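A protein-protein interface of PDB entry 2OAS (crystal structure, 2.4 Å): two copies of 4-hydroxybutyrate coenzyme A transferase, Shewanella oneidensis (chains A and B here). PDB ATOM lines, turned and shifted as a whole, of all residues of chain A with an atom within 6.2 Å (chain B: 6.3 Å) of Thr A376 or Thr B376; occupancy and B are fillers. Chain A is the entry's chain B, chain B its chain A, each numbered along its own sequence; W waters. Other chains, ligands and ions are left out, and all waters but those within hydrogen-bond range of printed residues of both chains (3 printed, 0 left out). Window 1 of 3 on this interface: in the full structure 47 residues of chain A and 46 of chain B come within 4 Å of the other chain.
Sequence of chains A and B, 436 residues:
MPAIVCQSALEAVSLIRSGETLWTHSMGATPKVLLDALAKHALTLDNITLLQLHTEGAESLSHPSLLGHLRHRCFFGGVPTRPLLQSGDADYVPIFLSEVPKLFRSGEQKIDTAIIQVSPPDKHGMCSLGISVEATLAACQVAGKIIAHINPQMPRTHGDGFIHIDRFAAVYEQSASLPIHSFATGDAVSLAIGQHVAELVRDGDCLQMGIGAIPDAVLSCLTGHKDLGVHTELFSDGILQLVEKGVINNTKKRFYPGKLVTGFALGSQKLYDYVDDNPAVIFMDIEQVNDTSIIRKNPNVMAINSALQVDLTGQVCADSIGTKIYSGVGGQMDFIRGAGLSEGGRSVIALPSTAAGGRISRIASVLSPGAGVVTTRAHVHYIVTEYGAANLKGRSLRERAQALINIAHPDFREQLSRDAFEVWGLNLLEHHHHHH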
ATOM      1  N   PHE A  96      10.076  22.661  -7.866  1.00  0.00           N
ATOM      2  CA  PHE A  96       9.935  23.885  -8.661  1.00  0.00           C
ATOM      3  C   PHE A  96       8.553  23.836  -9.266  1.00  0.00           C
ATOM      4  O   PHE A  96       8.074  22.766  -9.650  1.00  0.00           O
ATOM      5  CB  PHE A  96      10.967  23.959  -9.792  1.00  0.00           C
ATOM      6  CG  PHE A  96      12.373  23.915  -9.310  1.00  0.00           C
ATOM      7  CD1 PHE A  96      12.838  24.860  -8.402  1.00  0.00           C
ATOM      8  CD2 PHE A  96      13.213  22.878  -9.688  1.00  0.00           C
ATOM      9  CE1 PHE A  96      14.113  24.760  -7.860  1.00  0.00           C
ATOM     10  CE2 PHE A  96      14.494  22.770  -9.151  1.00  0.00           C
ATOM     11  CZ  PHE A  96      14.943  23.714  -8.236  1.00  0.00           C
ATOM     12  N   GLY A 314      24.531  35.417   1.492  1.00  0.00           N
ATOM     13  CA  GLY A 314      23.657  35.535   0.354  1.00  0.00           C
ATOM     14  C   GLY A 314      22.749  34.332   0.161  1.00  0.00           C
ATOM     15  O   GLY A 314      22.019  34.292  -0.827  1.00  0.00           O
ATOM     16  N   GLN A 315      22.780  33.343   1.054  1.00  0.00           N
ATOM     17  CA  GLN A 315      21.880  32.196   0.878  1.00  0.00           C
ATOM     18  C   GLN A 315      20.484  32.662   1.251  1.00  0.00           C
ATOM     19  O   GLN A 315      20.262  33.193   2.336  1.00  0.00           O
ATOM     20  CB  GLN A 315      22.278  30.998   1.745  1.00  0.00           C
ATOM     21  CG  GLN A 315      23.681  30.444   1.489  1.00  0.00           C
ATOM     22  CD  GLN A 315      23.875  29.057   2.084  1.00  0.00           C
ATOM     23  OE1 GLN A 315      23.409  28.056   1.538  1.00  0.00           O
ATOM     24  NE2 GLN A 315      24.560  28.997   3.231  1.00  0.00           N
ATOM     25  N   VAL A 316      19.542  32.450   0.341  1.00  0.00           N
ATOM     26  CA  VAL A 316      18.168  32.887   0.511  1.00  0.00           C
ATOM     27  C   VAL A 316      17.184  31.789   0.883  1.00  0.00           C
ATOM     28  O   VAL A 316      17.117  30.746   0.224  1.00  0.00           O
ATOM     29  CB  VAL A 316      17.689  33.559  -0.784  1.00  0.00           C
ATOM     30  CG1 VAL A 316      16.229  33.982  -0.665  1.00  0.00           C
ATOM     31  CG2 VAL A 316      18.583  34.747  -1.098  1.00  0.00           C
ATOM     32  N   MET A 333      13.447  31.184  -8.081  1.00  0.00           N
ATOM     33  CA  MET A 333      14.782  30.805  -8.495  1.00  0.00           C
ATOM     34  C   MET A 333      14.912  30.816 -10.014  1.00  0.00           C
ATOM     35  O   MET A 333      15.841  31.399 -10.568  1.00  0.00           O
ATOM     36  CB  MET A 333      15.121  29.430  -7.959  1.00  0.00           C
ATOM     37  CG  MET A 333      16.590  29.117  -8.063  1.00  0.00           C
ATOM     38  SD  MET A 333      16.945  27.253  -7.810  1.00  0.00           S
ATOM     39  CE  MET A 333      16.537  26.676  -9.621  1.00  0.00           C
ATOM     40  N   VAL A 373      16.643  26.324   1.797  1.00  0.00           N
ATOM     41  CA  VAL A 373      17.267  27.252   0.871  1.00  0.00           C
ATOM     42  C   VAL A 373      16.535  27.174  -0.465  1.00  0.00           C
ATOM     43  O   VAL A 373      16.510  26.114  -1.084  1.00  0.00           O
ATOM     44  CB  VAL A 373      18.731  26.888   0.631  1.00  0.00           C
ATOM     45  CG1 VAL A 373      19.270  27.673  -0.557  1.00  0.00           C
ATOM     46  CG2 VAL A 373      19.545  27.163   1.883  1.00  0.00           C
ATOM     47  N   VAL A 374      15.937  28.278  -0.911  1.00  0.00           N
ATOM     48  CA  VAL A 374      15.229  28.278  -2.195  1.00  0.00           C
ATOM     49  C   VAL A 374      16.153  28.801  -3.292  1.00  0.00           C
ATOM     50  O   VAL A 374      16.242  28.224  -4.375  1.00  0.00           O
ATOM     51  CB  VAL A 374      13.954  29.141  -2.133  1.00  0.00           C
ATOM     52  CG1 VAL A 374      13.257  29.156  -3.498  1.00  0.00           C
ATOM     53  CG2 VAL A 374      13.023  28.588  -1.077  1.00  0.00           C
ATOM     54  N   THR A 375      16.853  29.892  -2.987  1.00  0.00           N
ATOM     55  CA  THR A 375      17.788  30.513  -3.913  1.00  0.00           C
ATOM     56  C   THR A 375      19.165  30.477  -3.249  1.00  0.00           C
ATOM     57  O   THR A 375      19.319  30.885  -2.103  1.00  0.00           O
ATOM     58  CB  THR A 375      17.362  31.960  -4.205  1.00  0.00           C
ATOM     59  OG1 THR A 375      16.057  31.948  -4.800  1.00  0.00           O
ATOM     60  CG2 THR A 375      18.338  32.639  -5.146  1.00  0.00           C
ATOM     61  N   THR A 376      20.155  29.977  -3.980  1.00  0.00           N
ATOM     62  CA  THR A 376      21.504  29.840  -3.468  1.00  0.00           C
ATOM     63  C   THR A 376      22.392  31.077  -3.643  1.00  0.00           C
ATOM     64  O   THR A 376      22.026  32.028  -4.328  1.00  0.00           O
ATOM     65  CB  THR A 376      22.193  28.656  -4.149  1.00  0.00           C
ATOM     66  OG1 THR A 376      22.323  28.931  -5.552  1.00  0.00           O
ATOM     67  CG2 THR A 376      21.371  27.399  -3.968  1.00  0.00           C
ATOM     68  N   ARG A 377      23.561  31.048  -3.005  1.00  0.00           N
ATOM     69  CA  ARG A 377      24.549  32.116  -3.097  1.00  0.00           C
ATOM     70  C   ARG A 377      24.813  32.516  -4.537  1.00  0.00           C
ATOM     71  O   ARG A 377      24.680  33.669  -4.906  1.00  0.00           O
ATOM     72  CB  ARG A 377      25.897  31.650  -2.569  1.00  0.00           C
ATOM     73  CG  ARG A 377      25.971  31.321  -1.132  1.00  0.00           C
ATOM     74  CD  ARG A 377      27.275  30.588  -0.861  1.00  0.00           C
ATOM     75  NE  ARG A 377      27.535  30.555   0.568  1.00  0.00           N
ATOM     76  CZ  ARG A 377      28.366  29.721   1.163  1.00  0.00           C
ATOM     77  NH1 ARG A 377      29.040  28.819   0.459  1.00  0.00           N
ATOM     78  NH2 ARG A 377      28.514  29.790   2.478  1.00  0.00           N
ATOM     79  N   ALA A 378      25.235  31.545  -5.334  1.00  0.00           N
ATOM     80  CA  ALA A 378      25.576  31.784  -6.732  1.00  0.00           C
ATOM     81  C   ALA A 378      24.482  32.440  -7.546  1.00  0.00           C
ATOM     82  O   ALA A 378      24.774  33.098  -8.540  1.00  0.00           O
ATOM     83  CB  ALA A 378      26.004  30.470  -7.387  1.00  0.00           C
ATOM     84  N   HIS A 379      23.233  32.258  -7.116  1.00  0.00           N
ATOM     85  CA  HIS A 379      22.069  32.829  -7.798  1.00  0.00           C
ATOM     86  C   HIS A 379      21.882  34.315  -7.573  1.00  0.00           C
ATOM     87  O   HIS A 379      21.657  35.072  -8.514  1.00  0.00           O
ATOM     88  CB  HIS A 379      20.778  32.139  -7.345  1.00  0.00           C
ATOM     89  CG  HIS A 379      20.444  30.902  -8.113  1.00  0.00           C
ATOM     90  ND1 HIS A 379      20.472  29.643  -7.547  1.00  0.00           N
ATOM     91  CD2 HIS A 379      20.089  30.732  -9.411  1.00  0.00           C
ATOM     92  CE1 HIS A 379      20.149  28.750  -8.469  1.00  0.00           C
ATOM     93  NE2 HIS A 379      19.913  29.383  -9.609  1.00  0.00           N
ATOM     94  N   VAL A 380      21.967  34.724  -6.321  1.00  0.00           N
ATOM     95  CA  VAL A 380      21.722  36.105  -5.955  1.00  0.00           C
ATOM     96  C   VAL A 380      22.430  37.204  -6.735  1.00  0.00           C
ATOM     97  O   VAL A 380      23.595  37.090  -7.103  1.00  0.00           O
ATOM     98  CB  VAL A 380      21.977  36.304  -4.444  1.00  0.00           C
ATOM     99  CG1 VAL A 380      21.588  37.724  -4.032  1.00  0.00           C
ATOM    100  CG2 VAL A 380      21.167  35.282  -3.659  1.00  0.00           C
ATOM    101  N   ARG A 400      30.213  40.409   0.374  1.00  0.00           N
ATOM    102  CA  ARG A 400      28.789  40.145   0.496  1.00  0.00           C
ATOM    103  C   ARG A 400      28.310  40.460   1.908  1.00  0.00           C
ATOM    104  O   ARG A 400      27.327  41.181   2.107  1.00  0.00           O
ATOM    105  CB  ARG A 400      28.504  38.668   0.151  1.00  0.00           C
ATOM    106  CG  ARG A 400      28.834  38.287  -1.319  1.00  0.00           C
ATOM    107  CD  ARG A 400      29.030  36.768  -1.537  1.00  0.00           C
ATOM    108  NE  ARG A 400      27.796  36.056  -1.864  1.00  0.00           N
ATOM    109  CZ  ARG A 400      27.319  35.885  -3.093  1.00  0.00           C
ATOM    110  NH1 ARG A 400      27.970  36.372  -4.146  1.00  0.00           N
ATOM    111  NH2 ARG A 400      26.182  35.226  -3.270  1.00  0.00           N
ATOM    112  N   PHE B  96      28.238  30.047 -10.264  1.00  0.00           N
ATOM    113  CA  PHE B  96      28.114  28.873 -11.139  1.00  0.00           C
ATOM    114  C   PHE B  96      29.259  28.950 -12.126  1.00  0.00           C
ATOM    115  O   PHE B  96      29.631  30.035 -12.562  1.00  0.00           O
ATOM    116  CB  PHE B  96      26.782  28.861 -11.905  1.00  0.00           C
ATOM    117  CG  PHE B  96      25.587  28.872 -11.018  1.00  0.00           C
ATOM    118  CD1 PHE B  96      25.408  27.875 -10.070  1.00  0.00           C
ATOM    119  CD2 PHE B  96      24.697  29.935 -11.050  1.00  0.00           C
ATOM    120  CE1 PHE B  96      24.363  27.941  -9.153  1.00  0.00           C
ATOM    121  CE2 PHE B  96      23.649  30.010 -10.138  1.00  0.00           C
ATOM    122  CZ  PHE B  96      23.484  29.011  -9.185  1.00  0.00           C
ATOM    123  N   GLY B 314      16.992  16.562   2.053  1.00  0.00           N
ATOM    124  CA  GLY B 314      17.487  16.529   0.703  1.00  0.00           C
ATOM    125  C   GLY B 314      18.319  17.748   0.344  1.00  0.00           C
ATOM    126  O   GLY B 314      18.715  17.878  -0.810  1.00  0.00           O
ATOM    127  N   GLN B 315      18.571  18.665   1.284  1.00  0.00           N
ATOM    128  CA  GLN B 315      19.404  19.825   0.941  1.00  0.00           C
ATOM    129  C   GLN B 315      20.847  19.345   0.832  1.00  0.00           C
ATOM    130  O   GLN B 315      21.376  18.739   1.749  1.00  0.00           O
ATOM    131  CB  GLN B 315      19.304  20.947   1.980  1.00  0.00           C
ATOM    132  CG  GLN B 315      17.907  21.547   2.145  1.00  0.00           C
ATOM    133  CD  GLN B 315      17.932  22.882   2.879  1.00  0.00           C
ATOM    134  OE1 GLN B 315      18.247  23.917   2.298  1.00  0.00           O
ATOM    135  NE2 GLN B 315      17.605  22.857   4.180  1.00  0.00           N
ATOM    136  N   VAL B 316      21.468  19.622  -0.304  1.00  0.00           N
ATOM    137  CA  VAL B 316      22.820  19.186  -0.597  1.00  0.00           C
ATOM    138  C   VAL B 316      23.898  20.258  -0.463  1.00  0.00           C
ATOM    139  O   VAL B 316      23.796  21.349  -1.045  1.00  0.00           O
ATOM    140  CB  VAL B 316      22.867  18.619  -2.026  1.00  0.00           C
ATOM    141  CG1 VAL B 316      24.289  18.190  -2.400  1.00  0.00           C
ATOM    142  CG2 VAL B 316      21.894  17.450  -2.138  1.00  0.00           C
ATOM    143  N   MET B 333      24.789  21.538 -10.078  1.00  0.00           N
ATOM    144  CA  MET B 333      23.393  21.937 -10.040  1.00  0.00           C
ATOM    145  C   MET B 333      22.806  22.039 -11.441  1.00  0.00           C
ATOM    146  O   MET B 333      21.743  21.500 -11.729  1.00  0.00           O
ATOM    147  CB  MET B 333      23.258  23.270  -9.322  1.00  0.00           C
ATOM    148  CG  MET B 333      21.836  23.594  -8.952  1.00  0.00           C
ATOM    149  SD  MET B 333      21.651  25.453  -8.494  1.00  0.00           S
ATOM    150  CE  MET B 333      21.478  26.141 -10.281  1.00  0.00           C
ATOM    151  N   VAL B 373      24.798  25.631   0.650  1.00  0.00           N
ATOM    152  CA  VAL B 373      23.902  24.777  -0.115  1.00  0.00           C
ATOM    153  C   VAL B 373      24.217  24.968  -1.602  1.00  0.00           C
ATOM    154  O   VAL B 373      24.131  26.081  -2.109  1.00  0.00           O
ATOM    155  CB  VAL B 373      22.432  25.153   0.127  1.00  0.00           C
ATOM    156  CG1 VAL B 373      21.545  24.453  -0.897  1.00  0.00           C
ATOM    157  CG2 VAL B 373      22.033  24.792   1.532  1.00  0.00           C
ATOM    158  N   VAL B 374      24.596  23.899  -2.288  1.00  0.00           N
ATOM    159  CA  VAL B 374      24.898  23.996  -3.721  1.00  0.00           C
ATOM    160  C   VAL B 374      23.682  23.548  -4.533  1.00  0.00           C
ATOM    161  O   VAL B 374      23.301  24.191  -5.507  1.00  0.00           O
ATOM    162  CB  VAL B 374      26.120  23.122  -4.098  1.00  0.00           C
ATOM    163  CG1 VAL B 374      26.389  23.198  -5.603  1.00  0.00           C
ATOM    164  CG2 VAL B 374      27.340  23.604  -3.327  1.00  0.00           C
ATOM    165  N   THR B 375      23.073  22.446  -4.108  1.00  0.00           N
ATOM    166  CA  THR B 375      21.895  21.895  -4.757  1.00  0.00           C
ATOM    167  C   THR B 375      20.779  21.859  -3.711  1.00  0.00           C
ATOM    168  O   THR B 375      20.958  21.348  -2.612  1.00  0.00           O
ATOM    169  CB  THR B 375      22.187  20.481  -5.273  1.00  0.00           C
ATOM    170  OG1 THR B 375      23.246  20.544  -6.225  1.00  0.00           O
ATOM    171  CG2 THR B 375      20.966  19.878  -5.921  1.00  0.00           C
ATOM    172  N   THR B 376      19.625  22.400  -4.077  1.00  0.00           N
ATOM    173  CA  THR B 376      18.494  22.499  -3.174  1.00  0.00           C
ATOM    174  C   THR B 376      17.573  21.290  -3.158  1.00  0.00           C
ATOM    175  O   THR B 376      17.682  20.400  -3.998  1.00  0.00           O
ATOM    176  CB  THR B 376      17.669  23.737  -3.528  1.00  0.00           C
ATOM    177  OG1 THR B 376      17.113  23.578  -4.838  1.00  0.00           O
ATOM    178  CG2 THR B 376      18.557  24.974  -3.542  1.00  0.00           C
ATOM    179  N   ARG B 377      16.668  21.269  -2.180  1.00  0.00           N
ATOM    180  CA  ARG B 377      15.674  20.205  -2.037  1.00  0.00           C
ATOM    181  C   ARG B 377      14.996  19.902  -3.362  1.00  0.00           C
ATOM    182  O   ARG B 377      14.999  18.769  -3.834  1.00  0.00           O
ATOM    183  CB  ARG B 377      14.550  20.629  -1.107  1.00  0.00           C
ATOM    184  CG  ARG B 377      14.890  20.816   0.304  1.00  0.00           C
ATOM    185  CD  ARG B 377      13.735  21.501   1.005  1.00  0.00           C
ATOM    186  NE  ARG B 377      13.922  21.441   2.446  1.00  0.00           N
ATOM    187  CZ  ARG B 377      13.337  22.248   3.319  1.00  0.00           C
ATOM    188  NH1 ARG B 377      12.509  23.203   2.911  1.00  0.00           N
ATOM    189  NH2 ARG B 377      13.594  22.101   4.606  1.00  0.00           N
ATOM    190  N   ALA B 378      14.387  20.934  -3.935  1.00  0.00           N
ATOM    191  CA  ALA B 378      13.635  20.813  -5.187  1.00  0.00           C
ATOM    192  C   ALA B 378      14.419  20.214  -6.342  1.00  0.00           C
ATOM    193  O   ALA B 378      13.837  19.637  -7.256  1.00  0.00           O
ATOM    194  CB  ALA B 378      13.077  22.187  -5.582  1.00  0.00           C
ATOM    195  N   HIS B 379      15.740  20.361  -6.289  1.00  0.00           N
ATOM    196  CA  HIS B 379      16.631  19.843  -7.337  1.00  0.00           C
ATOM    197  C   HIS B 379      16.851  18.340  -7.283  1.00  0.00           C
ATOM    198  O   HIS B 379      16.771  17.658  -8.288  1.00  0.00           O
ATOM    199  CB  HIS B 379      18.008  20.497  -7.242  1.00  0.00           C
ATOM    200  CG  HIS B 379      18.123  21.788  -7.982  1.00  0.00           C
ATOM    201  ND1 HIS B 379      18.300  22.998  -7.348  1.00  0.00           N
ATOM    202  CD2 HIS B 379      18.057  22.061  -9.307  1.00  0.00           C
ATOM    203  CE1 HIS B 379      18.332  23.963  -8.250  1.00  0.00           C
ATOM    204  NE2 HIS B 379      18.186  23.421  -9.446  1.00  0.00           N
ATOM    205  N   VAL B 380      17.140  17.841  -6.098  1.00  0.00           N
ATOM    206  CA  VAL B 380      17.457  16.442  -5.926  1.00  0.00           C
ATOM    207  C   VAL B 380      16.521  15.400  -6.539  1.00  0.00           C
ATOM    208  O   VAL B 380      15.298  15.531  -6.532  1.00  0.00           O
ATOM    209  CB  VAL B 380      17.658  16.134  -4.420  1.00  0.00           C
ATOM    210  CG1 VAL B 380      18.113  14.696  -4.227  1.00  0.00           C
ATOM    211  CG2 VAL B 380      18.680  17.096  -3.842  1.00  0.00           C
ATOM    212  N   ARG B 400      11.138  11.637   2.329  1.00  0.00           N
ATOM    213  CA  ARG B 400      12.533  11.903   2.041  1.00  0.00           C
ATOM    214  C   ARG B 400      13.410  11.486   3.228  1.00  0.00           C
ATOM    215  O   ARG B 400      14.396  10.761   3.075  1.00  0.00           O
ATOM    216  CB  ARG B 400      12.732  13.402   1.741  1.00  0.00           C
ATOM    217  CG  ARG B 400      12.014  13.896   0.466  1.00  0.00           C
ATOM    218  CD  ARG B 400      11.799  15.423   0.445  1.00  0.00           C
ATOM    219  NE  ARG B 400      12.879  16.172  -0.196  1.00  0.00           N
ATOM    220  CZ  ARG B 400      12.961  16.430  -1.500  1.00  0.00           C
ATOM    221  NH1 ARG B 400      12.024  16.007  -2.337  1.00  0.00           N
ATOM    222  NH2 ARG B 400      13.991  17.119  -1.972  1.00  0.00           N
HETATM  223  O   HOH W   1      17.304  23.401  -0.611  1.00  0.00           O
HETATM  224  O   HOH W   2      24.618  26.649  -6.138  1.00  0.00           O
HETATM  225  O   HOH W   3      23.425  28.647  -1.561  1.00  0.00           O
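N of Val A373 sits at hydrogen-bond distance from OE1 of Gln B315, 2.9 Å away. The backbone NH of Val B373 sits at hydrogen-bond distance from the side-chain amide oxygen of Gln A315 (2.9 Å).
OG1 of Thr B376 is in hydrogen-bond range of ND1 of His B379, at 2.8 Å. OG1 of Thr A376 sits at hydrogen-bond distance from ND1 of His A379 (2.8 Å).
Among the printed residues, pairs that only touch across the chains: Phe A96 with Ala B378, Phe A96 with His B379, Met A333 with His B379, Val A373 with Val B373, Val A373 with Thr B376, Thr A376 with Phe B96, Thr A376 with Val B373, Thr A376 with Thr B376, Ala A378 with Phe B96, His A379 with Phe B96 and His A379 with Met B333.
Thr A376 touches three residues of chain B. Thr B376 touches just these residues of chain A: Val A373 and Thr A376. Of the printed residues of chain A, Met B333 touches His A379. Of the printed residues of chain B, Gln A315 touches Val B373. Of the printed residues of chain B, Ala A378 touches Phe B96 (3.4 Å). Arg B377 touches none of the printed residues of chain A. The nearest residue of chain A that does not touch Thr B376 is Phe A96 (4.03 Å). The nearest printed residue of chain A that does not touch Phe B96 is Arg A377 (6.0 Å).
Hydrophobic or aromatic side chains of chain B that line the printed part of chain A: Phe B96, Met B333, Val B373, Ala B378 and His B379. Of the 14 printed residues of chain A, 7 touch a printed residue of chain B. Printed residues of chain A that touch a printed residue of chain B: Phe A96, Gln A315, Met A333, Val A373, Thr A376, Ala A378 and His A379. Hydrophobic or aromatic side chains of chain A that line the printed part of chain B: Phe A96, Met A333, Val A373, Ala A378 and His A379.
Phe A96 touches His B379, and with the chains exchanged His A379 touches Phe B96. Val B373 touches its own counterpart, Val A373. Val A373 touches Thr B376, and with the chains exchanged Thr A376 touches Val B373. Thr A376 touches its own counterpart, Thr B376. Of the 13 pairs that touch across the chains among the printed residues, 12 have their exchanged pair printed and touching as well.
Water W3 lies within hydrogen-bond range of the backbone carbonyl oxygen of Val B373, the backbone NH of Arg A377 and the side-chain amide oxygen of Gln A315. Water W1 lies within hydrogen-bond range of N of Arg B377 (2.7 Å), O of Val A373 (2.9 Å) and OE1 of Gln B315 (3.1 Å). Water W2 lies within hydrogen-bond range of the backbone carbonyl oxygen (O) of Val B374 (2.9 Å) and the side-chain hydroxyl (OG1) of Thr A376 (3.3 Å).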
